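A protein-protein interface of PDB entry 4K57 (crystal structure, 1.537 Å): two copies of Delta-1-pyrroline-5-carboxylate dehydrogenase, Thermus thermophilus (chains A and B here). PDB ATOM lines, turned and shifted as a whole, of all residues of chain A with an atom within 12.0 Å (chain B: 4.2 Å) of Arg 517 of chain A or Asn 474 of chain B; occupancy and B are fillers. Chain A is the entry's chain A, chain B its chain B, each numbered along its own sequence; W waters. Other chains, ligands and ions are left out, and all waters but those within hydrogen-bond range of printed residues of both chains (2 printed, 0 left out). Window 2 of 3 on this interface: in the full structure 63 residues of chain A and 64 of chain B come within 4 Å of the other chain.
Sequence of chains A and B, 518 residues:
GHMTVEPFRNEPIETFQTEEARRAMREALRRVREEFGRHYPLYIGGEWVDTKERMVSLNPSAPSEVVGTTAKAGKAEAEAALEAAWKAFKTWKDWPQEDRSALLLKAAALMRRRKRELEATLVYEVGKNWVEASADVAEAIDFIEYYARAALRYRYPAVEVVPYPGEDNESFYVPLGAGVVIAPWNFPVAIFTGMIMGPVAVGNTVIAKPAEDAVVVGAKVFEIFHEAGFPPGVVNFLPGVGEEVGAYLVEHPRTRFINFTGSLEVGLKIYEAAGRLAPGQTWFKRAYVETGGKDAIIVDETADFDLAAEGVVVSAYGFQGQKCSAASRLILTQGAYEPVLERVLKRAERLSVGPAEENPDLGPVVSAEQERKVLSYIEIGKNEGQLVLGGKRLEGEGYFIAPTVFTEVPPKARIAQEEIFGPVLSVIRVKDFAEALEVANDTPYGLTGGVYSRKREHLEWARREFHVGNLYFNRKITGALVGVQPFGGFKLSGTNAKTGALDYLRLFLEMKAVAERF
The guanidinium group of Arg 475 of chain B is in salt-bridge range of the side-chain carboxylate of Glu 167 of chain A (2.8 Å). The backbone NH (N) of Phe 473 of chain B lies within hydrogen-bond range of the backbone carbonyl oxygen (O) of Ala 515 of chain A. The backbone NH of Arg 517 of chain A sits at hydrogen-bond distance from the backbone carbonyl oxygen of Phe 473 of chain B, 3.1 Å away.
The side-chain carboxylate of Glu 167 of chain A lies within hydrogen-bond range of the side-chain amide nitrogen of Asn 169 of chain A. The backbone NH (N) of Glu 516 of chain A is in hydrogen-bond range of the backbone carbonyl oxygen (O) of Asp 168 of chain A (2.9 Å). N of Val 514 of chain A is in hydrogen-bond range of O of Glu 170 of chain A, 2.8 Å away. N of Val 451 of chain B lies within hydrogen-bond range of O of Tyr 472 of chain B, 2.9 Å away. O of Arg 475 of chain B sits close to OH of Tyr 452 of chain B (3.4 Å). The side-chain amide nitrogen of Asn 474 of chain B lies within hydrogen-bond range of the backbone carbonyl oxygen of Ser 453 of chain B, at 2.9 Å.
CG1 of Val 514 of chain A touches CE2 of Phe 473 of chain B (3.6 Å). Ala 515 of chain A touches Tyr 472 of chain B. Phe 473 of chain B touches Glu 516 of chain A (O to CA, 3.6 Å). Arg 517 of chain A touches Asn 474 of chain B. Arg 517 of chain A touches Arg 475 of chain B.
Pro 163 of chain A touches none of the printed residues of chain B. Of the printed residues of chain B, Glu 167 of chain A touches Arg 475 (2.8 Å). Asp 168 of chain A touches none of the printed residues of chain B. Printed residues of chain B within 4 Å of Val 514 of chain A: Phe 473. Printed residues of chain B within 4 Å of Ala 515 of chain A: Tyr 472 (3.3 Å) and Phe 473 (2.7 Å). Of the printed residues of chain B, Glu 516 of chain A touches Phe 473. Of the printed residues of chain B, Arg 517 of chain A touches Phe 473, Asn 474 and Arg 475. No residue of chain A comes within 4 Å of Val 451 of chain B. No residue of chain A comes within 4 Å of Ser 453 of chain B. Printed residues of chain A within 4 Å of Tyr 472 of chain B: Ala 515 (3.3 Å). Of chain A, only Arg 517 (3.8 Å) comes within 4 Å of Asn 474 of chain B. Arg 475 of chain B touches just these residues of chain A: Glu 167 (2.8 Å) and Arg 517 (3.5 Å). The nearest printed residue of chain B that does not touch Arg 517 of chain A is Leu 307 of chain B (6.1 Å). The nearest printed residue of chain B that does not touch Glu 167 of chain A is Tyr 472 of chain B (6.0 Å).
Of the 8 printed residues of chain B, 4 touch a printed residue of chain A. Printed residues of chain B that touch a printed residue of chain A: Tyr 472, Phe 473, Asn 474 and Arg 475. Hydrophobic or aromatic side chains of chain B that line the printed part of chain A: Tyr 472 and Phe 473. Along chain B the printed residues that touch a printed residue of chain A span positions 472 to 475. Among the printed residues, Asp or Glu carboxylates within 4 Å of a Lys or Arg side-chain nitrogen of the other chain: Glu 167 of chain A with Arg 475 of chain B (2.8 Å).
No position is printed for both chains. Of the 8 pairs that touch across the chains among the printed residues, none has its exchanged pair printed and touching as well.
Water W2 lies within hydrogen-bond range of OE2 of Glu 516 of chain A (2.7 Å), O of Arg 517 of chain A (2.8 Å) and ND2 of Asn 474 of chain B (2.9 Å). Water W1 bridges OE2 of Glu 167 of chain A (2.8 Å) and NH1 of Arg 475 of chain B (3.0 Å).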
ATOM      1  N   VAL A 162     -29.511 -15.010 -24.450  1.00  0.00           N
ATOM      2  CA  VAL A 162     -29.110 -15.409 -25.791  1.00  0.00           C
ATOM      3  C   VAL A 162     -27.914 -16.337 -25.651  1.00  0.00           C
ATOM      4  O   VAL A 162     -26.918 -15.973 -25.031  1.00  0.00           O
ATOM      5  CB  VAL A 162     -28.672 -14.182 -26.620  1.00  0.00           C
ATOM      6  CG1 VAL A 162     -28.169 -14.601 -27.998  1.00  0.00           C
ATOM      7  CG2 VAL A 162     -29.814 -13.176 -26.730  1.00  0.00           C
ATOM      8  N   PRO A 163     -27.996 -17.550 -26.214  1.00  0.00           N
ATOM      9  CA  PRO A 163     -26.831 -18.433 -26.064  1.00  0.00           C
ATOM     10  C   PRO A 163     -25.639 -18.023 -26.928  1.00  0.00           C
ATOM     11  O   PRO A 163     -25.778 -17.250 -27.885  1.00  0.00           O
ATOM     12  CB  PRO A 163     -27.368 -19.808 -26.493  1.00  0.00           C
ATOM     13  CG  PRO A 163     -28.582 -19.513 -27.324  1.00  0.00           C
ATOM     14  CD  PRO A 163     -29.173 -18.244 -26.763  1.00  0.00           C
ATOM     15  N   TYR A 164     -24.460 -18.530 -26.584  1.00  0.00           N
ATOM     16  CA  TYR A 164     -23.256 -18.228 -27.324  1.00  0.00           C
ATOM     17  C   TYR A 164     -22.511 -19.532 -27.547  1.00  0.00           C
ATOM     18  O   TYR A 164     -22.457 -20.372 -26.656  1.00  0.00           O
ATOM     19  CB  TYR A 164     -22.382 -17.220 -26.553  1.00  0.00           C
ATOM     20  CG  TYR A 164     -21.150 -16.786 -27.313  1.00  0.00           C
ATOM     21  CD1 TYR A 164     -21.205 -15.741 -28.224  1.00  0.00           C
ATOM     22  CD2 TYR A 164     -19.932 -17.439 -27.134  1.00  0.00           C
ATOM     23  CE1 TYR A 164     -20.083 -15.353 -28.931  1.00  0.00           C
ATOM     24  CE2 TYR A 164     -18.801 -17.052 -27.833  1.00  0.00           C
ATOM     25  CZ  TYR A 164     -18.885 -16.008 -28.728  1.00  0.00           C
ATOM     26  OH  TYR A 164     -17.758 -15.631 -29.430  1.00  0.00           O
ATOM     27  N   PRO A 165     -21.950 -19.721 -28.741  1.00  0.00           N
ATOM     28  CA  PRO A 165     -21.297 -20.999 -29.044  1.00  0.00           C
ATOM     29  C   PRO A 165     -20.155 -21.344 -28.097  1.00  0.00           C
ATOM     30  O   PRO A 165     -19.308 -20.490 -27.808  1.00  0.00           O
ATOM     31  CB  PRO A 165     -20.719 -20.767 -30.445  1.00  0.00           C
ATOM     32  CG  PRO A 165     -21.600 -19.718 -31.041  1.00  0.00           C
ATOM     33  CD  PRO A 165     -21.995 -18.822 -29.907  1.00  0.00           C
ATOM     34  N   GLY A 166     -20.131 -22.593 -27.638  1.00  0.00           N
ATOM     35  CA  GLY A 166     -19.020 -23.100 -26.852  1.00  0.00           C
ATOM     36  C   GLY A 166     -19.037 -22.629 -25.411  1.00  0.00           C
ATOM     37  O   GLY A 166     -18.036 -22.777 -24.700  1.00  0.00           O
ATOM     38  N   GLU A 167     -20.162 -22.062 -24.991  1.00  0.00           N
ATOM     39  CA  GLU A 167     -20.287 -21.461 -23.666  1.00  0.00           C
ATOM     40  C   GLU A 167     -21.566 -21.859 -22.992  1.00  0.00           C
ATOM     41  O   GLU A 167     -22.580 -22.089 -23.655  1.00  0.00           O
ATOM     42  CB  GLU A 167     -20.299 -19.931 -23.757  1.00  0.00           C
ATOM     43  CG  GLU A 167     -18.970 -19.302 -23.978  1.00  0.00           C
ATOM     44  CD  GLU A 167     -18.981 -17.800 -23.707  1.00  0.00           C
ATOM     45  OE1 GLU A 167     -17.876 -17.225 -23.662  1.00  0.00           O
ATOM     46  OE2 GLU A 167     -20.074 -17.210 -23.555  1.00  0.00           O
ATOM     47  N   ASP A 168     -21.526 -21.905 -21.660  1.00  0.00           N
ATOM     48  CA  ASP A 168     -22.728 -22.012 -20.841  1.00  0.00           C
ATOM     49  C   ASP A 168     -22.927 -20.654 -20.187  1.00  0.00           C
ATOM     50  O   ASP A 168     -22.035 -20.158 -19.506  1.00  0.00           O
ATOM     51  CB  ASP A 168     -22.532 -23.109 -19.774  1.00  0.00           C
ATOM     52  CG  ASP A 168     -23.713 -23.241 -18.814  1.00  0.00           C
ATOM     53  OD1 ASP A 168     -23.563 -23.953 -17.803  1.00  0.00           O
ATOM     54  OD2 ASP A 168     -24.779 -22.648 -19.048  1.00  0.00           O
ATOM     55  N   ASN A 169     -24.083 -20.041 -20.410  1.00  0.00           N
ATOM     56  CA  ASN A 169     -24.366 -18.738 -19.826  1.00  0.00           C
ATOM     57  C   ASN A 169     -25.587 -18.818 -18.927  1.00  0.00           C
ATOM     58  O   ASN A 169     -26.683 -19.103 -19.391  1.00  0.00           O
ATOM     59  CB  ASN A 169     -24.558 -17.687 -20.929  1.00  0.00           C
ATOM     60  CG  ASN A 169     -23.249 -17.200 -21.483  1.00  0.00           C
ATOM     61  OD1 ASN A 169     -22.580 -16.357 -20.868  1.00  0.00           O
ATOM     62  ND2 ASN A 169     -22.845 -17.742 -22.635  1.00  0.00           N
ATOM     63  N   GLU A 170     -25.370 -18.590 -17.632  1.00  0.00           N
ATOM     64  CA  GLU A 170     -26.419 -18.733 -16.618  1.00  0.00           C
ATOM     65  C   GLU A 170     -26.656 -17.403 -15.916  1.00  0.00           C
ATOM     66  O   GLU A 170     -25.743 -16.836 -15.322  1.00  0.00           O
ATOM     67  CB  GLU A 170     -26.009 -19.785 -15.581  1.00  0.00           C
ATOM     68  CG  GLU A 170     -25.629 -21.151 -16.162  1.00  0.00           C
ATOM     69  CD  GLU A 170     -25.414 -22.213 -15.089  1.00  0.00           C
ATOM     70  OE1 GLU A 170     -25.664 -21.918 -13.901  1.00  0.00           O
ATOM     71  OE2 GLU A 170     -24.989 -23.340 -15.435  1.00  0.00           O
ATOM     72  N   ALA A 513     -24.701 -13.002 -13.501  1.00  0.00           N
ATOM     73  CA  ALA A 513     -24.516 -13.701 -14.779  1.00  0.00           C
ATOM     74  C   ALA A 513     -23.194 -14.438 -14.745  1.00  0.00           C
ATOM     75  O   ALA A 513     -22.144 -13.825 -14.536  1.00  0.00           O
ATOM     76  CB  ALA A 513     -24.549 -12.729 -15.932  1.00  0.00           C
ATOM     77  N   VAL A 514     -23.238 -15.751 -14.977  1.00  0.00           N
ATOM     78  CA  VAL A 514     -22.028 -16.571 -14.922  1.00  0.00           C
ATOM     79  C   VAL A 514     -21.820 -17.255 -16.255  1.00  0.00           C
ATOM     80  O   VAL A 514     -22.719 -17.919 -16.763  1.00  0.00           O
ATOM     81  CB  VAL A 514     -22.131 -17.631 -13.813  1.00  0.00           C
ATOM     82  CG1 VAL A 514     -20.819 -18.405 -13.678  1.00  0.00           C
ATOM     83  CG2 VAL A 514     -22.512 -16.960 -12.488  1.00  0.00           C
ATOM     84  N   ALA A 515     -20.637 -17.078 -16.826  1.00  0.00           N
ATOM     85  CA  ALA A 515     -20.325 -17.630 -18.139  1.00  0.00           C
ATOM     86  C   ALA A 515     -19.140 -18.584 -18.052  1.00  0.00           C
ATOM     87  O   ALA A 515     -18.077 -18.206 -17.562  1.00  0.00           O
ATOM     88  CB  ALA A 515     -19.992 -16.505 -19.106  1.00  0.00           C
ATOM     89  N   GLU A 516     -19.310 -19.814 -18.535  1.00  0.00           N
ATOM     90  CA  GLU A 516     -18.174 -20.731 -18.662  1.00  0.00           C
ATOM     91  C   GLU A 516     -17.869 -21.014 -20.128  1.00  0.00           C
ATOM     92  O   GLU A 516     -18.756 -21.429 -20.881  1.00  0.00           O
ATOM     93  CB  GLU A 516     -18.428 -22.066 -17.946  1.00  0.00           C
ATOM     94  CG  GLU A 516     -17.271 -23.037 -18.160  1.00  0.00           C
ATOM     95  CD  GLU A 516     -17.413 -24.360 -17.427  1.00  0.00           C
ATOM     96  OE1 GLU A 516     -18.447 -24.583 -16.757  1.00  0.00           O
ATOM     97  OE2 GLU A 516     -16.466 -25.171 -17.541  1.00  0.00           O
ATOM     98  N   ARG A 517     -16.621 -20.807 -20.516  1.00  0.00           N
ATOM     99  CA  ARG A 517     -16.147 -21.199 -21.842  1.00  0.00           C
ATOM    100  C   ARG A 517     -15.521 -22.583 -21.725  1.00  0.00           C
ATOM    101  O   ARG A 517     -14.555 -22.789 -20.977  1.00  0.00           O
ATOM    102  CB  ARG A 517     -15.130 -20.183 -22.388  1.00  0.00           C
ATOM    103  CG  ARG A 517     -14.618 -20.497 -23.792  1.00  0.00           C
ATOM    104  CD  ARG A 517     -15.600 -20.059 -24.880  1.00  0.00           C
ATOM    105  NE  ARG A 517     -15.905 -18.627 -24.825  1.00  0.00           N
ATOM    106  CZ  ARG A 517     -15.102 -17.668 -25.278  1.00  0.00           C
ATOM    107  NH1 ARG A 517     -13.928 -17.977 -25.808  1.00  0.00           N
ATOM    108  NH2 ARG A 517     -15.466 -16.394 -25.195  1.00  0.00           N
ATOM    109  N   PHE A 518     -16.073 -23.538 -22.466  1.00  0.00           N
ATOM    110  CA  PHE A 518     -15.617 -24.928 -22.367  1.00  0.00           C
ATOM    111  C   PHE A 518     -14.355 -25.224 -23.138  1.00  0.00           C
ATOM    112  O   PHE A 518     -13.657 -26.195 -22.827  1.00  0.00           O
ATOM    113  CB  PHE A 518     -16.736 -25.879 -22.804  1.00  0.00           C
ATOM    114  CG  PHE A 518     -17.934 -25.826 -21.921  1.00  0.00           C
ATOM    115  CD1 PHE A 518     -19.132 -25.296 -22.382  1.00  0.00           C
ATOM    116  CD2 PHE A 518     -17.868 -26.290 -20.604  1.00  0.00           C
ATOM    117  CE1 PHE A 518     -20.251 -25.234 -21.562  1.00  0.00           C
ATOM    118  CE2 PHE A 518     -18.979 -26.241 -19.774  1.00  0.00           C
ATOM    119  CZ  PHE A 518     -20.176 -25.707 -20.248  1.00  0.00           C
ATOM    120  OXT PHE A 518     -13.993 -24.506 -24.070  1.00  0.00           O
ATOM    121  N   LEU B 307      -3.745 -20.697 -21.362  1.00  0.00           N
ATOM    122  CA  LEU B 307      -5.050 -20.101 -21.610  1.00  0.00           C
ATOM    123  C   LEU B 307      -5.273 -18.951 -20.634  1.00  0.00           C
ATOM    124  O   LEU B 307      -5.734 -17.868 -21.014  1.00  0.00           O
ATOM    125  CB  LEU B 307      -6.160 -21.152 -21.466  1.00  0.00           C
ATOM    126  CG  LEU B 307      -7.558 -20.734 -21.909  1.00  0.00           C
ATOM    127  CD1 LEU B 307      -7.634 -20.660 -23.432  1.00  0.00           C
ATOM    128  CD2 LEU B 307      -8.601 -21.710 -21.363  1.00  0.00           C
ATOM    129  N   VAL B 451     -12.345 -16.801 -13.126  1.00  0.00           N
ATOM    130  CA  VAL B 451     -11.603 -17.901 -12.522  1.00  0.00           C
ATOM    131  C   VAL B 451     -11.101 -18.801 -13.628  1.00  0.00           C
ATOM    132  O   VAL B 451     -11.895 -19.277 -14.451  1.00  0.00           O
ATOM    133  CB  VAL B 451     -12.489 -18.769 -11.596  1.00  0.00           C
ATOM    134  CG1 VAL B 451     -11.665 -19.931 -11.038  1.00  0.00           C
ATOM    135  CG2 VAL B 451     -13.077 -17.939 -10.458  1.00  0.00           C
ATOM    136  N   TYR B 452      -9.787 -19.005 -13.673  1.00  0.00           N
ATOM    137  CA  TYR B 452      -9.219 -20.073 -14.483  1.00  0.00           C
ATOM    138  C   TYR B 452      -8.908 -21.254 -13.581  1.00  0.00           C
ATOM    139  O   TYR B 452      -8.077 -21.168 -12.673  1.00  0.00           O
ATOM    140  CB  TYR B 452      -7.963 -19.609 -15.221  1.00  0.00           C
ATOM    141  CG  TYR B 452      -8.268 -18.791 -16.451  1.00  0.00           C
ATOM    142  CD1 TYR B 452      -8.467 -17.419 -16.357  1.00  0.00           C
ATOM    143  CD2 TYR B 452      -8.340 -19.381 -17.710  1.00  0.00           C
ATOM    144  CE1 TYR B 452      -8.742 -16.656 -17.476  1.00  0.00           C
ATOM    145  CE2 TYR B 452      -8.615 -18.623 -18.841  1.00  0.00           C
ATOM    146  CZ  TYR B 452      -8.820 -17.265 -18.716  1.00  0.00           C
ATOM    147  OH  TYR B 452      -9.092 -16.503 -19.832  1.00  0.00           O
ATOM    148  N   SER B 453      -9.602 -22.355 -13.834  1.00  0.00           N
ATOM    149  CA  SER B 453      -9.470 -23.571 -13.039  1.00  0.00           C
ATOM    150  C   SER B 453     -10.121 -24.697 -13.813  1.00  0.00           C
ATOM    151  O   SER B 453     -11.121 -24.474 -14.503  1.00  0.00           O
ATOM    152  CB  SER B 453     -10.198 -23.412 -11.703  1.00  0.00           C
ATOM    153  OG  SER B 453     -10.148 -24.612 -10.943  1.00  0.00           O
ATOM    154  N   TYR B 472     -16.858 -15.006 -14.917  1.00  0.00           N
ATOM    155  CA  TYR B 472     -16.454 -15.769 -16.085  1.00  0.00           C
ATOM    156  C   TYR B 472     -15.495 -16.880 -15.722  1.00  0.00           C
ATOM    157  O   TYR B 472     -14.558 -16.665 -14.966  1.00  0.00           O
ATOM    158  CB  TYR B 472     -15.772 -14.844 -17.098  1.00  0.00           C
ATOM    159  CG  TYR B 472     -16.665 -13.730 -17.595  1.00  0.00           C
ATOM    160  CD1 TYR B 472     -16.699 -12.510 -16.935  1.00  0.00           C
ATOM    161  CD2 TYR B 472     -17.467 -13.899 -18.724  1.00  0.00           C
ATOM    162  CE1 TYR B 472     -17.495 -11.479 -17.384  1.00  0.00           C
ATOM    163  CE2 TYR B 472     -18.267 -12.875 -19.177  1.00  0.00           C
ATOM    164  CZ  TYR B 472     -18.277 -11.674 -18.500  1.00  0.00           C
ATOM    165  OH  TYR B 472     -19.079 -10.649 -18.933  1.00  0.00           O
ATOM    166  N   PHE B 473     -15.725 -18.065 -16.281  1.00  0.00           N
ATOM    167  CA  PHE B 473     -14.843 -19.203 -16.037  1.00  0.00           C
ATOM    168  C   PHE B 473     -14.065 -19.552 -17.301  1.00  0.00           C
ATOM    169  O   PHE B 473     -14.660 -19.808 -18.361  1.00  0.00           O
ATOM    170  CB  PHE B 473     -15.652 -20.436 -15.590  1.00  0.00           C
ATOM    171  CG  PHE B 473     -16.413 -20.250 -14.300  1.00  0.00           C
ATOM    172  CD1 PHE B 473     -15.979 -19.353 -13.334  1.00  0.00           C
ATOM    173  CD2 PHE B 473     -17.569 -20.982 -14.061  1.00  0.00           C
ATOM    174  CE1 PHE B 473     -16.685 -19.197 -12.139  1.00  0.00           C
ATOM    175  CE2 PHE B 473     -18.286 -20.831 -12.876  1.00  0.00           C
ATOM    176  CZ  PHE B 473     -17.840 -19.932 -11.913  1.00  0.00           C
ATOM    177  N   ASN B 474     -12.739 -19.540 -17.172  1.00  0.00           N
ATOM    178  CA  ASN B 474     -11.823 -19.968 -18.233  1.00  0.00           C
ATOM    179  C   ASN B 474     -11.933 -19.168 -19.522  1.00  0.00           C
ATOM    180  O   ASN B 474     -11.804 -19.713 -20.617  1.00  0.00           O
ATOM    181  CB  ASN B 474     -11.963 -21.473 -18.479  1.00  0.00           C
ATOM    182  CG  ASN B 474     -11.533 -22.280 -17.284  1.00  0.00           C
ATOM    183  OD1 ASN B 474     -10.516 -21.974 -16.662  1.00  0.00           O
ATOM    184  ND2 ASN B 474     -12.315 -23.292 -16.925  1.00  0.00           N
ATOM    185  N   ARG B 475     -12.154 -17.867 -19.364  1.00  0.00           N
ATOM    186  CA  ARG B 475     -12.158 -16.920 -20.473  1.00  0.00           C
ATOM    187  C   ARG B 475     -11.985 -15.504 -19.946  1.00  0.00           C
ATOM    188  O   ARG B 475     -12.025 -15.265 -18.734  1.00  0.00           O
ATOM    189  CB  ARG B 475     -13.452 -17.025 -21.275  1.00  0.00           C
ATOM    190  CG  ARG B 475     -14.699 -16.929 -20.413  1.00  0.00           C
ATOM    191  CD  ARG B 475     -15.830 -16.347 -21.235  1.00  0.00           C
ATOM    192  NE  ARG B 475     -15.659 -14.904 -21.362  1.00  0.00           N
ATOM    193  CZ  ARG B 475     -16.427 -14.114 -22.102  1.00  0.00           C
ATOM    194  NH1 ARG B 475     -17.416 -14.630 -22.822  1.00  0.00           N
ATOM    195  NH2 ARG B 475     -16.190 -12.801 -22.124  1.00  0.00           N
HETATM  196  O   HOH W   1     -19.591 -14.818 -24.932  1.00  0.00           O
HETATM  197  O   HOH W   2     -14.225 -24.401 -18.747  1.00  0.00           O
